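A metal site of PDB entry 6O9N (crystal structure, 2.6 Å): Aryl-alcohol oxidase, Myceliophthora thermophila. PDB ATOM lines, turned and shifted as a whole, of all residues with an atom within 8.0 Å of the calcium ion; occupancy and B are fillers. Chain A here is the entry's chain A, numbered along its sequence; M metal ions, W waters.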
ATOM      1  N   PRO A  75      36.451  15.897 -22.926  1.00  0.00           N
ATOM      2  CA  PRO A  75      35.033  15.904 -22.550  1.00  0.00           C
ATOM      3  C   PRO A  75      34.813  15.188 -21.229  1.00  0.00           C
ATOM      4  O   PRO A  75      35.442  14.163 -20.947  1.00  0.00           O
ATOM      5  CB  PRO A  75      34.348  15.154 -23.702  1.00  0.00           C
ATOM      6  CG  PRO A  75      35.300  15.225 -24.827  1.00  0.00           C
ATOM      7  CD  PRO A  75      36.677  15.270 -24.236  1.00  0.00           C
ATOM      8  N   GLY A  76      33.958  15.758 -20.398  1.00  0.00           N
ATOM      9  CA  GLY A  76      33.555  15.074 -19.199  1.00  0.00           C
ATOM     10  C   GLY A  76      32.636  13.910 -19.514  1.00  0.00           C
ATOM     11  O   GLY A  76      32.159  13.715 -20.638  1.00  0.00           O
ATOM     12  N   THR A  77      32.401  13.087 -18.498  1.00  0.00           N
ATOM     13  CA  THR A  77      31.395  12.043 -18.618  1.00  0.00           C
ATOM     14  C   THR A  77      30.010  12.678 -18.823  1.00  0.00           C
ATOM     15  O   THR A  77      29.705  13.709 -18.227  1.00  0.00           O
ATOM     16  CB  THR A  77      31.444  11.175 -17.369  1.00  0.00           C
ATOM     17  OG1 THR A  77      32.762  10.649 -17.248  1.00  0.00           O
ATOM     18  CG2 THR A  77      30.470  10.043 -17.444  1.00  0.00           C
ATOM     19  N   PHE A  78      29.205  12.082 -19.688  1.00  0.00           N
ATOM     20  CA  PHE A  78      27.864  12.583 -20.017  1.00  0.00           C
ATOM     21  C   PHE A  78      27.896  14.103 -20.248  1.00  0.00           C
ATOM     22  O   PHE A  78      27.362  14.890 -19.471  1.00  0.00           O
ATOM     23  CB  PHE A  78      26.879  12.195 -18.903  1.00  0.00           C
ATOM     24  CG  PHE A  78      25.441  12.565 -19.179  1.00  0.00           C
ATOM     25  CD1 PHE A  78      24.794  12.118 -20.317  1.00  0.00           C
ATOM     26  CD2 PHE A  78      24.735  13.347 -18.271  1.00  0.00           C
ATOM     27  CE1 PHE A  78      23.475  12.453 -20.563  1.00  0.00           C
ATOM     28  CE2 PHE A  78      23.398  13.689 -18.526  1.00  0.00           C
ATOM     29  CZ  PHE A  78      22.778  13.249 -19.670  1.00  0.00           C
ATOM     30  N   ASP A  79      28.578  14.503 -21.307  1.00  0.00           N
ATOM     31  CA  ASP A  79      28.619  15.876 -21.808  1.00  0.00           C
ATOM     32  C   ASP A  79      27.981  15.877 -23.186  1.00  0.00           C
ATOM     33  O   ASP A  79      27.746  14.812 -23.774  1.00  0.00           O
ATOM     34  CB  ASP A  79      30.067  16.400 -21.865  1.00  0.00           C
ATOM     35  CG  ASP A  79      30.616  16.783 -20.492  1.00  0.00           C
ATOM     36  OD1 ASP A  79      30.025  16.363 -19.484  1.00  0.00           O
ATOM     37  OD2 ASP A  79      31.636  17.515 -20.391  1.00  0.00           O
ATOM     38  N   PRO A  80      27.647  17.047 -23.730  1.00  0.00           N
ATOM     39  CA  PRO A  80      26.984  17.059 -25.035  1.00  0.00           C
ATOM     40  C   PRO A  80      27.836  16.337 -26.061  1.00  0.00           C
ATOM     41  O   PRO A  80      29.080  16.321 -25.963  1.00  0.00           O
ATOM     42  CB  PRO A  80      26.861  18.558 -25.350  1.00  0.00           C
ATOM     43  CG  PRO A  80      26.784  19.201 -24.026  1.00  0.00           C
ATOM     44  CD  PRO A  80      27.655  18.376 -23.090  1.00  0.00           C
ATOM     45  N   THR A  82      25.885  13.504 -25.771  1.00  0.00           N
ATOM     46  CA  THR A  82      25.550  12.169 -25.387  1.00  0.00           C
ATOM     47  C   THR A  82      24.238  11.883 -24.709  1.00  0.00           C
ATOM     48  O   THR A  82      23.544  12.732 -24.271  1.00  0.00           O
ATOM     49  CB  THR A  82      26.690  11.610 -24.519  1.00  0.00           C
ATOM     50  OG1 THR A  82      26.800  12.364 -23.340  1.00  0.00           O
ATOM     51  CG2 THR A  82      27.962  11.691 -25.242  1.00  0.00           C
ATOM     52  N   TRP A  84      22.291   9.116 -21.767  1.00  0.00           N
ATOM     53  CA  TRP A  84      22.756   8.548 -20.511  1.00  0.00           C
ATOM     54  C   TRP A  84      23.623   7.339 -20.631  1.00  0.00           C
ATOM     55  O   TRP A  84      23.245   6.228 -20.887  1.00  0.00           O
ATOM     56  CB  TRP A  84      21.769   8.573 -19.369  1.00  0.00           C
ATOM     57  CG  TRP A  84      22.362   8.163 -18.094  1.00  0.00           C
ATOM     58  CD1 TRP A  84      22.244   6.972 -17.527  1.00  0.00           C
ATOM     59  CD2 TRP A  84      23.164   8.932 -17.213  1.00  0.00           C
ATOM     60  NE1 TRP A  84      22.899   6.915 -16.387  1.00  0.00           N
ATOM     61  CE2 TRP A  84      23.476   8.111 -16.139  1.00  0.00           C
ATOM     62  CE3 TRP A  84      23.653  10.230 -17.231  1.00  0.00           C
ATOM     63  CZ2 TRP A  84      24.232   8.531 -15.084  1.00  0.00           C
ATOM     64  CZ3 TRP A  84      24.412  10.636 -16.174  1.00  0.00           C
ATOM     65  CH2 TRP A  84      24.698   9.791 -15.112  1.00  0.00           C
ATOM     66  N   GLN A  88      31.622   9.771 -25.661  1.00  0.00           N
ATOM     67  CA  GLN A  88      31.853  11.093 -26.171  1.00  0.00           C
ATOM     68  C   GLN A  88      32.504  11.040 -27.533  1.00  0.00           C
ATOM     69  O   GLN A  88      33.555  10.488 -27.686  1.00  0.00           O
ATOM     70  CB  GLN A  88      32.698  11.891 -25.230  1.00  0.00           C
ATOM     71  CG  GLN A  88      32.128  11.904 -23.851  1.00  0.00           C
ATOM     72  CD  GLN A  88      30.941  12.780 -23.704  1.00  0.00           C
ATOM     73  OE1 GLN A  88      30.685  13.622 -24.523  1.00  0.00           O
ATOM     74  NE2 GLN A  88      30.229  12.608 -22.657  1.00  0.00           N
ATOM     75  N   MET A 127      35.113  10.255 -13.596  1.00  0.00           N
ATOM     76  CA  MET A 127      35.058  11.463 -12.765  1.00  0.00           C
ATOM     77  C   MET A 127      34.465  11.275 -11.382  1.00  0.00           C
ATOM     78  O   MET A 127      34.277  12.262 -10.670  1.00  0.00           O
ATOM     79  CB  MET A 127      34.344  12.605 -13.492  1.00  0.00           C
ATOM     80  CG  MET A 127      34.988  12.879 -14.849  1.00  0.00           C
ATOM     81  SD  MET A 127      34.099  13.984 -15.955  1.00  0.00           S
ATOM     82  CE  MET A 127      33.933  15.449 -14.954  1.00  0.00           C
ATOM     83  N   PRO A 202      27.399  18.265  -8.990  1.00  0.00           N
ATOM     84  CA  PRO A 202      26.619  18.820 -10.100  1.00  0.00           C
ATOM     85  C   PRO A 202      25.372  19.531  -9.588  1.00  0.00           C
ATOM     86  O   PRO A 202      24.890  19.293  -8.481  1.00  0.00           O
ATOM     87  CB  PRO A 202      26.250  17.580 -10.930  1.00  0.00           C
ATOM     88  CG  PRO A 202      27.285  16.592 -10.585  1.00  0.00           C
ATOM     89  CD  PRO A 202      27.566  16.809  -9.124  1.00  0.00           C
ATOM     90  N   ALA A 240      32.141  15.088  -8.209  1.00  0.00           N
ATOM     91  CA  ALA A 240      32.712  14.935  -9.538  1.00  0.00           C
ATOM     92  C   ALA A 240      33.994  15.754  -9.642  1.00  0.00           C
ATOM     93  O   ALA A 240      34.088  16.836  -9.067  1.00  0.00           O
ATOM     94  CB  ALA A 240      31.729  15.360 -10.631  1.00  0.00           C
ATOM     95  N   GLN A 242      35.320  18.058 -11.418  1.00  0.00           N
ATOM     96  CA  GLN A 242      34.849  19.001 -12.430  1.00  0.00           C
ATOM     97  C   GLN A 242      34.643  20.361 -11.815  1.00  0.00           C
ATOM     98  O   GLN A 242      34.458  20.507 -10.607  1.00  0.00           O
ATOM     99  CB  GLN A 242      33.555  18.528 -13.100  1.00  0.00           C
ATOM    100  CG  GLN A 242      32.335  18.504 -12.170  1.00  0.00           C
ATOM    101  CD  GLN A 242      31.068  18.163 -12.944  1.00  0.00           C
ATOM    102  OE1 GLN A 242      31.030  17.187 -13.695  1.00  0.00           O
ATOM    103  NE2 GLN A 242      30.024  18.985 -12.787  1.00  0.00           N
ATOM    104  N   THR A 246      31.352  25.718 -14.355  1.00  0.00           N
ATOM    105  CA  THR A 246      31.168  25.325 -15.742  1.00  0.00           C
ATOM    106  C   THR A 246      30.886  23.838 -15.924  1.00  0.00           C
ATOM    107  O   THR A 246      30.496  23.432 -17.029  1.00  0.00           O
ATOM    108  CB  THR A 246      32.396  25.714 -16.554  1.00  0.00           C
ATOM    109  OG1 THR A 246      33.463  24.805 -16.241  1.00  0.00           O
ATOM    110  CG2 THR A 246      32.840  27.092 -16.189  1.00  0.00           C
ATOM    111  N   ALA A 247      31.062  23.023 -14.892  1.00  0.00           N
ATOM    112  CA  ALA A 247      30.900  21.575 -14.946  1.00  0.00           C
ATOM    113  C   ALA A 247      31.872  20.916 -15.931  1.00  0.00           C
ATOM    114  O   ALA A 247      31.675  19.744 -16.285  1.00  0.00           O
ATOM    115  CB  ALA A 247      29.450  21.172 -15.285  1.00  0.00           C
ATOM    116  N   ARG A 248      32.917  21.625 -16.378  1.00  0.00           N
ATOM    117  CA  ARG A 248      33.864  21.042 -17.314  1.00  0.00           C
ATOM    118  C   ARG A 248      34.853  20.169 -16.552  1.00  0.00           C
ATOM    119  O   ARG A 248      35.217  20.469 -15.411  1.00  0.00           O
ATOM    120  CB  ARG A 248      34.598  22.133 -18.112  1.00  0.00           C
ATOM    121  CG  ARG A 248      33.658  23.072 -18.916  1.00  0.00           C
ATOM    122  CD  ARG A 248      33.060  22.396 -20.170  1.00  0.00           C
ATOM    123  NE  ARG A 248      32.349  23.299 -21.095  1.00  0.00           N
ATOM    124  CZ  ARG A 248      31.104  23.775 -20.927  1.00  0.00           C
ATOM    125  NH1 ARG A 248      30.394  23.484 -19.835  1.00  0.00           N
ATOM    126  NH2 ARG A 248      30.571  24.566 -21.847  1.00  0.00           N
ATOM    127  N   ARG A 249      35.266  19.067 -17.182  1.00  0.00           N
ATOM    128  CA  ARG A 249      36.131  18.088 -16.533  1.00  0.00           C
ATOM    129  C   ARG A 249      37.389  18.745 -15.990  1.00  0.00           C
ATOM    130  O   ARG A 249      38.036  19.540 -16.671  1.00  0.00           O
ATOM    131  CB  ARG A 249      36.519  16.984 -17.531  1.00  0.00           C
ATOM    132  CG  ARG A 249      37.384  15.890 -16.952  1.00  0.00           C
ATOM    133  CD  ARG A 249      38.050  15.051 -18.048  1.00  0.00           C
ATOM    134  NE  ARG A 249      37.145  14.111 -18.702  1.00  0.00           N
ATOM    135  CZ  ARG A 249      36.763  12.947 -18.191  1.00  0.00           C
ATOM    136  NH1 ARG A 249      37.202  12.556 -16.989  1.00  0.00           N
ATOM    137  NH2 ARG A 249      35.934  12.159 -18.868  1.00  0.00           N
ATOM    138  N   PHE A 391      24.294  23.422 -20.799  1.00  0.00           N
ATOM    139  CA  PHE A 391      25.683  23.164 -20.477  1.00  0.00           C
ATOM    140  C   PHE A 391      26.586  24.341 -20.865  1.00  0.00           C
ATOM    141  O   PHE A 391      27.660  24.522 -20.275  1.00  0.00           O
ATOM    142  CB  PHE A 391      26.113  21.877 -21.174  1.00  0.00           C
ATOM    143  CG  PHE A 391      27.410  21.311 -20.669  1.00  0.00           C
ATOM    144  CD1 PHE A 391      27.517  20.858 -19.351  1.00  0.00           C
ATOM    145  CD2 PHE A 391      28.511  21.243 -21.499  1.00  0.00           C
ATOM    146  CE1 PHE A 391      28.723  20.336 -18.872  1.00  0.00           C
ATOM    147  CE2 PHE A 391      29.705  20.721 -21.040  1.00  0.00           C
ATOM    148  CZ  PHE A 391      29.827  20.275 -19.714  1.00  0.00           C
ATOM    149  N   GLY A 398      21.699  21.915 -15.952  1.00  0.00           N
ATOM    150  CA  GLY A 398      20.982  20.797 -16.525  1.00  0.00           C
ATOM    151  C   GLY A 398      21.750  19.494 -16.590  1.00  0.00           C
ATOM    152  O   GLY A 398      22.899  19.395 -16.160  1.00  0.00           O
ATOM    153  N   PRO A 399      21.114  18.477 -17.186  1.00  0.00           N
ATOM    154  CA  PRO A 399      21.616  17.089 -17.129  1.00  0.00           C
ATOM    155  C   PRO A 399      23.122  16.904 -17.337  1.00  0.00           C
ATOM    156  O   PRO A 399      23.766  16.099 -16.649  1.00  0.00           O
ATOM    157  CB  PRO A 399      20.865  16.403 -18.273  1.00  0.00           C
ATOM    158  CG  PRO A 399      19.619  17.195 -18.441  1.00  0.00           C
ATOM    159  CD  PRO A 399      19.948  18.615 -18.077  1.00  0.00           C
ATOM    160  N   TYR A 400      23.698  17.633 -18.293  1.00  0.00           N
ATOM    161  CA  TYR A 400      25.091  17.381 -18.624  1.00  0.00           C
ATOM    162  C   TYR A 400      26.044  17.840 -17.536  1.00  0.00           C
ATOM    163  O   TYR A 400      27.213  17.463 -17.558  1.00  0.00           O
ATOM    164  CB  TYR A 400      25.429  18.062 -19.957  1.00  0.00           C
ATOM    165  CG  TYR A 400      24.874  17.359 -21.180  1.00  0.00           C
ATOM    166  CD1 TYR A 400      25.085  16.005 -21.405  1.00  0.00           C
ATOM    167  CD2 TYR A 400      24.141  18.067 -22.123  1.00  0.00           C
ATOM    168  CE1 TYR A 400      24.568  15.365 -22.544  1.00  0.00           C
ATOM    169  CE2 TYR A 400      23.632  17.459 -23.260  1.00  0.00           C
ATOM    170  CZ  TYR A 400      23.856  16.106 -23.456  1.00  0.00           C
ATOM    171  OH  TYR A 400      23.343  15.511 -24.595  1.00  0.00           O
ATOM    172  N   THR A 401      25.592  18.657 -16.582  1.00  0.00           N
ATOM    173  CA  THR A 401      26.485  18.992 -15.469  1.00  0.00           C
ATOM    174  C   THR A 401      26.770  17.760 -14.625  1.00  0.00           C
ATOM    175  O   THR A 401      27.735  17.760 -13.857  1.00  0.00           O
ATOM    176  CB  THR A 401      25.882  20.090 -14.581  1.00  0.00           C
ATOM    177  OG1 THR A 401      24.628  19.654 -14.056  1.00  0.00           O
ATOM    178  CG2 THR A 401      25.673  21.390 -15.369  1.00  0.00           C
ATOM    179  N   LEU A 402      25.951  16.737 -14.758  1.00  0.00           N
ATOM    180  CA  LEU A 402      26.171  15.466 -14.092  1.00  0.00           C
ATOM    181  C   LEU A 402      27.323  14.721 -14.778  1.00  0.00           C
ATOM    182  O   LEU A 402      27.452  14.757 -16.005  1.00  0.00           O
ATOM    183  CB  LEU A 402      24.883  14.668 -14.167  1.00  0.00           C
ATOM    184  CG  LEU A 402      24.481  13.488 -13.309  1.00  0.00           C
ATOM    185  CD1 LEU A 402      24.784  13.721 -11.834  1.00  0.00           C
ATOM    186  CD2 LEU A 402      23.005  13.294 -13.554  1.00  0.00           C
ATOM    187  N   ALA A 403      28.167  14.074 -13.979  1.00  0.00           N
ATOM    188  CA  ALA A 403      29.179  13.182 -14.550  1.00  0.00           C
ATOM    189  C   ALA A 403      28.580  11.781 -14.648  1.00  0.00           C
ATOM    190  O   ALA A 403      27.614  11.577 -15.385  1.00  0.00           O
ATOM    191  CB  ALA A 403      30.460  13.186 -13.718  1.00  0.00           C
ATOM    192  N   GLY A 404      29.094  10.808 -13.895  1.00  0.00           N
ATOM    193  CA  GLY A 404      28.509   9.487 -13.940  1.00  0.00           C
ATOM    194  C   GLY A 404      27.568   9.154 -12.792  1.00  0.00           C
ATOM    195  O   GLY A 404      27.028   8.046 -12.754  1.00  0.00           O
HETATM  196 CA    CA M   1      28.679  15.813 -17.690  1.00  0.00          CA
HETATM  197  O   HOH W   1      30.324  16.431 -16.020  1.00  0.00           O
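The side-chain hydroxyl (OH) of Tyr 400 sits at hydrogen-bond distance from the backbone carbonyl oxygen (O) of Thr 82 (2.8 Å).
The backbone NH of Gly 76 lies within hydrogen-bond range of the side-chain carboxylate of Asp 79 (2.9 Å).
The backbone NH (N) of Asp 79 lies close to the side-chain amide nitrogen (NE2) of Gln 88, 2.9 Å away.
The backbone NH (N) of Phe 78 lies close to the side-chain amide nitrogen (NE2) of Gln 88, at 3.2 Å.
The backbone NH of Thr 77 lies within hydrogen-bond range of the side-chain sulfur of Met 127 (3.2 Å).
O of Asp 79 is in hydrogen-bond range of OG1 of Thr 82 (2.7 Å).
The nearest printed residue that does not touch the calcium ion is Thr 401 (4.1 Å).
The calcium ion is bound by O of Tyr 400 (2.2 Å), OD1 of Asp 79 (2.3 Å), O of Leu 402 (2.3 Å), O of Phe 78 (2.4 Å), O of Thr 77 (2.4 Å) and water W1 (2.4 Å).
The calcium ion has six donor atoms within binding distance.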
